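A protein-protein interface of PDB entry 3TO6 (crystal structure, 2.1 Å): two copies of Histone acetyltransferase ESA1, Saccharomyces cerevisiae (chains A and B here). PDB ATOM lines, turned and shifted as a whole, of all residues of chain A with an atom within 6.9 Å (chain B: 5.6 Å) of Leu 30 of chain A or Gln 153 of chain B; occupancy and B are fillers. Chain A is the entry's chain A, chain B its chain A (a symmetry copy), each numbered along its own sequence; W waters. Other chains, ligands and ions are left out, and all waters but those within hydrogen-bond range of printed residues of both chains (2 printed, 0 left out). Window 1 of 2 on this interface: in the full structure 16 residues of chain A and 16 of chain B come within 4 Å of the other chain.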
ATOM      1  N   ARG A   4      14.165  -5.387  28.069  1.00  0.00           N
ATOM      2  CA  ARG A   4      14.726  -4.994  26.781  1.00  0.00           C
ATOM      3  C   ARG A   4      14.505  -6.044  25.696  1.00  0.00           C
ATOM      4  O   ARG A   4      14.753  -7.224  25.898  1.00  0.00           O
ATOM      5  CB  ARG A   4      16.217  -4.706  26.914  1.00  0.00           C
ATOM      6  CG  ARG A   4      16.533  -3.531  27.826  1.00  0.00           C
ATOM      7  CD  ARG A   4      17.459  -2.561  27.114  1.00  0.00           C
ATOM      8  NE  ARG A   4      18.855  -2.946  27.256  1.00  0.00           N
ATOM      9  CZ  ARG A   4      19.851  -2.441  26.534  1.00  0.00           C
ATOM     10  NH1 ARG A   4      19.618  -1.547  25.585  1.00  0.00           N
ATOM     11  NH2 ARG A   4      21.088  -2.846  26.754  1.00  0.00           N
ATOM     12  N   VAL A   5      14.060  -5.590  24.534  1.00  0.00           N
ATOM     13  CA  VAL A   5      13.778  -6.464  23.407  1.00  0.00           C
ATOM     14  C   VAL A   5      14.614  -5.955  22.247  1.00  0.00           C
ATOM     15  O   VAL A   5      14.205  -5.044  21.532  1.00  0.00           O
ATOM     16  CB  VAL A   5      12.267  -6.424  23.054  1.00  0.00           C
ATOM     17  CG1 VAL A   5      11.960  -7.279  21.830  1.00  0.00           C
ATOM     18  CG2 VAL A   5      11.437  -6.884  24.245  1.00  0.00           C
ATOM     19  N   ARG A   6      15.796  -6.539  22.071  1.00  0.00           N
ATOM     20  CA  ARG A   6      16.815  -5.955  21.197  1.00  0.00           C
ATOM     21  C   ARG A   6      16.814  -6.505  19.789  1.00  0.00           C
ATOM     22  O   ARG A   6      16.399  -7.628  19.556  1.00  0.00           O
ATOM     23  CB  ARG A   6      18.203  -6.160  21.797  1.00  0.00           C
ATOM     24  CG  ARG A   6      18.444  -5.350  23.051  1.00  0.00           C
ATOM     25  CD  ARG A   6      19.301  -4.150  22.704  1.00  0.00           C
ATOM     26  NE  ARG A   6      20.581  -4.216  23.376  1.00  0.00           N
ATOM     27  CZ  ARG A   6      21.612  -3.419  23.119  1.00  0.00           C
ATOM     28  NH1 ARG A   6      21.535  -2.482  22.180  1.00  0.00           N
ATOM     29  NH2 ARG A   6      22.727  -3.565  23.813  1.00  0.00           N
ATOM     30  N   ASN A   7      17.309  -5.692  18.865  1.00  0.00           N
ATOM     31  CA  ASN A   7      17.532  -6.093  17.488  1.00  0.00           C
ATOM     32  C   ASN A   7      18.917  -6.756  17.399  1.00  0.00           C
ATOM     33  O   ASN A   7      19.715  -6.663  18.332  1.00  0.00           O
ATOM     34  CB  ASN A   7      17.459  -4.843  16.598  1.00  0.00           C
ATOM     35  CG  ASN A   7      17.403  -5.163  15.114  1.00  0.00           C
ATOM     36  OD1 ASN A   7      17.147  -6.302  14.705  1.00  0.00           O
ATOM     37  ND2 ASN A   7      17.641  -4.149  14.297  1.00  0.00           N
ATOM     38  N   LEU A   8      19.200  -7.435  16.297  1.00  0.00           N
ATOM     39  CA  LEU A   8      20.526  -8.010  16.090  1.00  0.00           C
ATOM     40  C   LEU A   8      21.483  -6.915  15.610  1.00  0.00           C
ATOM     41  O   LEU A   8      21.432  -6.496  14.454  1.00  0.00           O
ATOM     42  CB  LEU A   8      20.461  -9.150  15.071  1.00  0.00           C
ATOM     43  CG  LEU A   8      21.775  -9.863  14.723  1.00  0.00           C
ATOM     44  CD1 LEU A   8      22.357 -10.513  15.955  1.00  0.00           C
ATOM     45  CD2 LEU A   8      21.570 -10.912  13.621  1.00  0.00           C
ATOM     46  N   PHE A  23      18.399  -5.793   8.087  1.00  0.00           N
ATOM     47  CA  PHE A  23      17.764  -6.853   8.856  1.00  0.00           C
ATOM     48  C   PHE A  23      17.767  -8.182   8.110  1.00  0.00           C
ATOM     49  O   PHE A  23      17.602  -8.218   6.889  1.00  0.00           O
ATOM     50  CB  PHE A  23      16.317  -6.464   9.151  1.00  0.00           C
ATOM     51  CG  PHE A  23      15.568  -7.497   9.923  1.00  0.00           C
ATOM     52  CD1 PHE A  23      15.532  -7.453  11.312  1.00  0.00           C
ATOM     53  CD2 PHE A  23      14.900  -8.512   9.269  1.00  0.00           C
ATOM     54  CE1 PHE A  23      14.841  -8.419  12.036  1.00  0.00           C
ATOM     55  CE2 PHE A  23      14.210  -9.477   9.980  1.00  0.00           C
ATOM     56  CZ  PHE A  23      14.179  -9.431  11.365  1.00  0.00           C
ATOM     57  N   ILE A  28      15.424 -16.574  15.552  1.00  0.00           N
ATOM     58  CA  ILE A  28      15.913 -16.555  16.924  1.00  0.00           C
ATOM     59  C   ILE A  28      14.991 -15.725  17.816  1.00  0.00           C
ATOM     60  O   ILE A  28      14.278 -14.845  17.336  1.00  0.00           O
ATOM     61  CB  ILE A  28      17.308 -15.909  16.984  1.00  0.00           C
ATOM     62  CG1 ILE A  28      17.256 -14.483  16.412  1.00  0.00           C
ATOM     63  CG2 ILE A  28      18.323 -16.754  16.206  1.00  0.00           C
ATOM     64  CD1 ILE A  28      18.615 -13.781  16.370  1.00  0.00           C
ATOM     65  N   GLU A  29      15.032 -15.982  19.120  1.00  0.00           N
ATOM     66  CA  GLU A  29      14.265 -15.181  20.067  1.00  0.00           C
ATOM     67  C   GLU A  29      14.900 -13.806  20.268  1.00  0.00           C
ATOM     68  O   GLU A  29      16.118 -13.688  20.334  1.00  0.00           O
ATOM     69  CB  GLU A  29      14.157 -15.892  21.420  1.00  0.00           C
ATOM     70  CG  GLU A  29      12.978 -15.392  22.252  1.00  0.00           C
ATOM     71  CD  GLU A  29      13.028 -15.835  23.706  1.00  0.00           C
ATOM     72  OE1 GLU A  29      14.011 -16.498  24.105  1.00  0.00           O
ATOM     73  OE2 GLU A  29      12.076 -15.512  24.450  1.00  0.00           O
ATOM     74  N   LEU A  30      14.074 -12.766  20.360  1.00  0.00           N
ATOM     75  CA  LEU A  30      14.564 -11.437  20.725  1.00  0.00           C
ATOM     76  C   LEU A  30      14.773 -11.388  22.233  1.00  0.00           C
ATOM     77  O   LEU A  30      13.893 -11.776  22.989  1.00  0.00           O
ATOM     78  CB  LEU A  30      13.546 -10.365  20.332  1.00  0.00           C
ATOM     79  CG  LEU A  30      13.058 -10.351  18.883  1.00  0.00           C
ATOM     80  CD1 LEU A  30      11.876  -9.389  18.729  1.00  0.00           C
ATOM     81  CD2 LEU A  30      14.198  -9.978  17.952  1.00  0.00           C
ATOM     82  N   THR A  31      15.938 -10.927  22.673  1.00  0.00           N
ATOM     83  CA  THR A  31      16.252 -10.904  24.096  1.00  0.00           C
ATOM     84  C   THR A  31      16.881  -9.578  24.466  1.00  0.00           C
ATOM     85  O   THR A  31      16.897  -8.629  23.669  1.00  0.00           O
ATOM     86  CB  THR A  31      17.256 -12.022  24.472  1.00  0.00           C
ATOM     87  OG1 THR A  31      18.530 -11.741  23.882  1.00  0.00           O
ATOM     88  CG2 THR A  31      16.768 -13.387  23.985  1.00  0.00           C
ATOM     89  N   ASP A  32      17.429  -9.512  25.671  1.00  0.00           N
ATOM     90  CA  ASP A  32      18.068  -8.288  26.116  1.00  0.00           C
ATOM     91  C   ASP A  32      19.514  -8.173  25.623  1.00  0.00           C
ATOM     92  O   ASP A  32      20.202  -7.204  25.934  1.00  0.00           O
ATOM     93  CB  ASP A  32      17.975  -8.138  27.641  1.00  0.00           C
ATOM     94  CG  ASP A  32      18.722  -9.227  28.384  1.00  0.00           C
ATOM     95  OD1 ASP A  32      19.070  -9.000  29.556  1.00  0.00           O
ATOM     96  OD2 ASP A  32      18.965 -10.306  27.802  1.00  0.00           O
ATOM     97  N   GLU A  33      19.958  -9.151  24.841  1.00  0.00           N
ATOM     98  CA  GLU A  33      21.277  -9.101  24.217  1.00  0.00           C
ATOM     99  C   GLU A  33      21.133  -8.830  22.722  1.00  0.00           C
ATOM    100  O   GLU A  33      20.086  -9.107  22.140  1.00  0.00           O
ATOM    101  CB  GLU A  33      22.029 -10.414  24.453  1.00  0.00           C
ATOM    102  CG  GLU A  33      22.255 -10.726  25.931  1.00  0.00           C
ATOM    103  CD  GLU A  33      22.893 -12.080  26.152  1.00  0.00           C
ATOM    104  OE1 GLU A  33      22.706 -12.978  25.305  1.00  0.00           O
ATOM    105  OE2 GLU A  33      23.594 -12.248  27.167  1.00  0.00           O
ATOM    106  N   TRP B  21      13.249  -2.489  13.790  1.00  0.00           N
ATOM    107  CA  TRP B  21      13.998  -3.209  12.763  1.00  0.00           C
ATOM    108  C   TRP B  21      14.180  -2.326  11.532  1.00  0.00           C
ATOM    109  O   TRP B  21      15.149  -2.477  10.792  1.00  0.00           O
ATOM    110  CB  TRP B  21      13.251  -4.482  12.318  1.00  0.00           C
ATOM    111  CG  TRP B  21      12.909  -5.464  13.419  1.00  0.00           C
ATOM    112  CD1 TRP B  21      13.319  -5.422  14.726  1.00  0.00           C
ATOM    113  CD2 TRP B  21      12.080  -6.631  13.296  1.00  0.00           C
ATOM    114  NE1 TRP B  21      12.790  -6.492  15.422  1.00  0.00           N
ATOM    115  CE2 TRP B  21      12.029  -7.247  14.567  1.00  0.00           C
ATOM    116  CE3 TRP B  21      11.367  -7.206  12.239  1.00  0.00           C
ATOM    117  CZ2 TRP B  21      11.295  -8.414  14.806  1.00  0.00           C
ATOM    118  CZ3 TRP B  21      10.642  -8.376  12.480  1.00  0.00           C
ATOM    119  CH2 TRP B  21      10.618  -8.964  13.753  1.00  0.00           C
ATOM    120  N   PHE B  99       8.563  -2.610  12.019  1.00  0.00           N
ATOM    121  CA  PHE B  99       8.916  -4.023  11.924  1.00  0.00           C
ATOM    122  C   PHE B  99       8.615  -4.622  10.543  1.00  0.00           C
ATOM    123  O   PHE B  99       8.591  -5.843  10.368  1.00  0.00           O
ATOM    124  CB  PHE B  99       8.224  -4.783  13.066  1.00  0.00           C
ATOM    125  CG  PHE B  99       8.426  -4.115  14.403  1.00  0.00           C
ATOM    126  CD1 PHE B  99       7.401  -3.401  15.003  1.00  0.00           C
ATOM    127  CD2 PHE B  99       9.669  -4.139  15.012  1.00  0.00           C
ATOM    128  CE1 PHE B  99       7.604  -2.748  16.212  1.00  0.00           C
ATOM    129  CE2 PHE B  99       9.882  -3.491  16.221  1.00  0.00           C
ATOM    130  CZ  PHE B  99       8.843  -2.789  16.816  1.00  0.00           C
ATOM    131  N   LEU B 147       0.937  -8.804  11.961  1.00  0.00           N
ATOM    132  CA  LEU B 147       2.036  -8.495  12.877  1.00  0.00           C
ATOM    133  C   LEU B 147       1.770  -9.032  14.281  1.00  0.00           C
ATOM    134  O   LEU B 147       0.673  -8.855  14.807  1.00  0.00           O
ATOM    135  CB  LEU B 147       2.197  -6.977  12.988  1.00  0.00           C
ATOM    136  CG  LEU B 147       3.146  -6.486  14.083  1.00  0.00           C
ATOM    137  CD1 LEU B 147       4.591  -6.660  13.596  1.00  0.00           C
ATOM    138  CD2 LEU B 147       2.872  -5.024  14.467  1.00  0.00           C
ATOM    139  N   THR B 148       2.767  -9.678  14.887  1.00  0.00           N
ATOM    140  CA  THR B 148       2.781  -9.886  16.336  1.00  0.00           C
ATOM    141  C   THR B 148       3.805  -8.915  16.904  1.00  0.00           C
ATOM    142  O   THR B 148       4.929  -8.848  16.405  1.00  0.00           O
ATOM    143  CB  THR B 148       3.187 -11.323  16.704  1.00  0.00           C
ATOM    144  OG1 THR B 148       2.188 -12.233  16.220  1.00  0.00           O
ATOM    145  CG2 THR B 148       3.310 -11.476  18.220  1.00  0.00           C
ATOM    146  N   LEU B 149       3.424  -8.126  17.907  1.00  0.00           N
ATOM    147  CA  LEU B 149       4.379  -7.193  18.506  1.00  0.00           C
ATOM    148  C   LEU B 149       5.612  -7.968  18.950  1.00  0.00           C
ATOM    149  O   LEU B 149       5.493  -9.094  19.430  1.00  0.00           O
ATOM    150  CB  LEU B 149       3.748  -6.421  19.678  1.00  0.00           C
ATOM    151  CG  LEU B 149       2.522  -5.557  19.335  1.00  0.00           C
ATOM    152  CD1 LEU B 149       1.934  -4.873  20.580  1.00  0.00           C
ATOM    153  CD2 LEU B 149       2.874  -4.513  18.277  1.00  0.00           C
ATOM    154  N   PRO B 150       6.811  -7.373  18.789  1.00  0.00           N
ATOM    155  CA  PRO B 150       8.056  -8.130  18.986  1.00  0.00           C
ATOM    156  C   PRO B 150       8.182  -8.707  20.387  1.00  0.00           C
ATOM    157  O   PRO B 150       8.707  -9.809  20.529  1.00  0.00           O
ATOM    158  CB  PRO B 150       9.163  -7.086  18.751  1.00  0.00           C
ATOM    159  CG  PRO B 150       8.494  -5.979  18.000  1.00  0.00           C
ATOM    160  CD  PRO B 150       7.066  -5.961  18.462  1.00  0.00           C
ATOM    161  N   GLN B 151       7.717  -7.977  21.399  1.00  0.00           N
ATOM    162  CA  GLN B 151       7.820  -8.452  22.776  1.00  0.00           C
ATOM    163  C   GLN B 151       6.983  -9.714  22.999  1.00  0.00           C
ATOM    164  O   GLN B 151       7.173 -10.420  23.986  1.00  0.00           O
ATOM    165  CB  GLN B 151       7.450  -7.349  23.791  1.00  0.00           C
ATOM    166  CG  GLN B 151       6.002  -6.854  23.746  1.00  0.00           C
ATOM    167  CD  GLN B 151       5.816  -5.679  22.806  1.00  0.00           C
ATOM    168  OE1 GLN B 151       6.413  -5.634  21.736  1.00  0.00           O
ATOM    169  NE2 GLN B 151       5.000  -4.711  23.211  1.00  0.00           N
ATOM    170  N   TYR B 152       6.078 -10.007  22.064  1.00  0.00           N
ATOM    171  CA  TYR B 152       5.218 -11.187  22.176  1.00  0.00           C
ATOM    172  C   TYR B 152       5.447 -12.251  21.102  1.00  0.00           C
ATOM    173  O   TYR B 152       4.688 -13.223  21.024  1.00  0.00           O
ATOM    174  CB  TYR B 152       3.739 -10.776  22.179  1.00  0.00           C
ATOM    175  CG  TYR B 152       3.363  -9.829  23.298  1.00  0.00           C
ATOM    176  CD1 TYR B 152       2.870  -8.560  23.020  1.00  0.00           C
ATOM    177  CD2 TYR B 152       3.519 -10.197  24.635  1.00  0.00           C
ATOM    178  CE1 TYR B 152       2.525  -7.678  24.040  1.00  0.00           C
ATOM    179  CE2 TYR B 152       3.167  -9.315  25.672  1.00  0.00           C
ATOM    180  CZ  TYR B 152       2.673  -8.063  25.360  1.00  0.00           C
ATOM    181  OH  TYR B 152       2.330  -7.180  26.360  1.00  0.00           O
ATOM    182  N   GLN B 153       6.480 -12.080  20.277  1.00  0.00           N
ATOM    183  CA  GLN B 153       6.710 -13.005  19.148  1.00  0.00           C
ATOM    184  C   GLN B 153       7.167 -14.402  19.600  1.00  0.00           C
ATOM    185  O   GLN B 153       7.705 -14.558  20.683  1.00  0.00           O
ATOM    186  CB  GLN B 153       7.707 -12.398  18.129  1.00  0.00           C
ATOM    187  CG  GLN B 153       7.046 -11.392  17.164  1.00  0.00           C
ATOM    188  CD  GLN B 153       8.035 -10.628  16.262  1.00  0.00           C
ATOM    189  OE1 GLN B 153       7.650  -9.690  15.560  1.00  0.00           O
ATOM    190  NE2 GLN B 153       9.292 -11.042  16.267  1.00  0.00           N
ATOM    191  N   ARG B 154       6.931 -15.413  18.772  1.00  0.00           N
ATOM    192  CA  ARG B 154       7.352 -16.777  19.068  1.00  0.00           C
ATOM    193  C   ARG B 154       6.677 -17.342  20.317  1.00  0.00           C
ATOM    194  O   ARG B 154       7.296 -18.091  21.078  1.00  0.00           O
ATOM    195  CB  ARG B 154       8.884 -16.877  19.200  1.00  0.00           C
ATOM    196  CG  ARG B 154       9.649 -16.421  17.957  1.00  0.00           C
ATOM    197  CD  ARG B 154      11.139 -16.818  18.043  1.00  0.00           C
ATOM    198  NE  ARG B 154      11.591 -17.343  16.762  1.00  0.00           N
ATOM    199  CZ  ARG B 154      11.703 -18.632  16.471  1.00  0.00           C
ATOM    200  NH1 ARG B 154      11.440 -19.553  17.380  1.00  0.00           N
ATOM    201  NH2 ARG B 154      12.107 -18.998  15.268  1.00  0.00           N
ATOM    202  N   MET B 155       5.410 -16.989  20.510  1.00  0.00           N
ATOM    203  CA  MET B 155       4.603 -17.517  21.612  1.00  0.00           C
ATOM    204  C   MET B 155       3.341 -18.198  21.066  1.00  0.00           C
ATOM    205  O   MET B 155       2.477 -18.613  21.837  1.00  0.00           O
ATOM    206  CB  MET B 155       4.203 -16.394  22.585  1.00  0.00           C
ATOM    207  CG  MET B 155       5.375 -15.706  23.290  1.00  0.00           C
ATOM    208  SD  MET B 155       4.859 -14.405  24.440  1.00  0.00           S
ATOM    209  CE  MET B 155       3.929 -15.356  25.643  1.00  0.00           C
ATOM    210  N   GLY B 156       3.229 -18.298  19.741  1.00  0.00           N
ATOM    211  CA  GLY B 156       2.045 -18.872  19.110  1.00  0.00           C
ATOM    212  C   GLY B 156       0.930 -17.901  18.689  1.00  0.00           C
ATOM    213  O   GLY B 156      -0.068 -18.314  18.097  1.00  0.00           O
HETATM  214  O   HOH W   1      13.576  -5.756  18.273  1.00  0.00           O
HETATM  215  O   HOH W   2      17.575  -4.050  11.510  1.00  0.00           O
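No position is printed for both chains.
Of the 5 pairs that touch across the chains among the printed residues, none has its exchanged pair printed and touching as well.
Water W2 bridges ND2 of Asn 7 of chain A and O of Trp 21 of chain B.
Water W1 bridges NE1 of Trp 21 of chain B and O of Val 5 of chain A.
Printed residues of chain A that touch a printed residue of chain B: Asn 7, Phe 23, Ile 28 and Leu 30.
Hydrophobic or aromatic side chains of chain A that line the printed part of chain B: Phe 23 and Leu 30.
Printed residues of chain B that touch a printed residue of chain A: Trp 21, Pro 150, Gln 153 and Arg 154.
Among the printed residues, 5 pairs touch across the chains.
The side-chain amide oxygen (OE1) of Gln 153 of chain B sits close to the backbone carbonyl oxygen (O) of Thr 148 of chain B (3.0 Å).
Among the printed residues, merely in contact across the chains: Asn 7 of chain A with Trp 21 of chain B, Phe 23 of chain A with Trp 21 of chain B, Ile 28 of chain A with Arg 154 of chain B, Leu 30 of chain A with Pro 150 of chain B and Leu 30 of chain A with Gln 153 of chain B.
Of chain B, only Pro 150 (3.6 Å) and Gln 153 (3.9 Å) come within 4 Å of Leu 30 of chain A.
Gln 153 of chain B touches just one residue of chain A: Leu 30.
Of the printed residues of chain B, Asn 7 of chain A touches Trp 21 (3.9 Å).
Of the printed residues of chain B, Ile 28 of chain A touches Arg 154.
The nearest residue of chain A that does not touch Gln 153 of chain B is Glu 29 of chain A (5.6 Å).
The nearest printed residue of chain B that does not touch Ile 28 of chain A is Gln 153 of chain B (6.4 Å).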
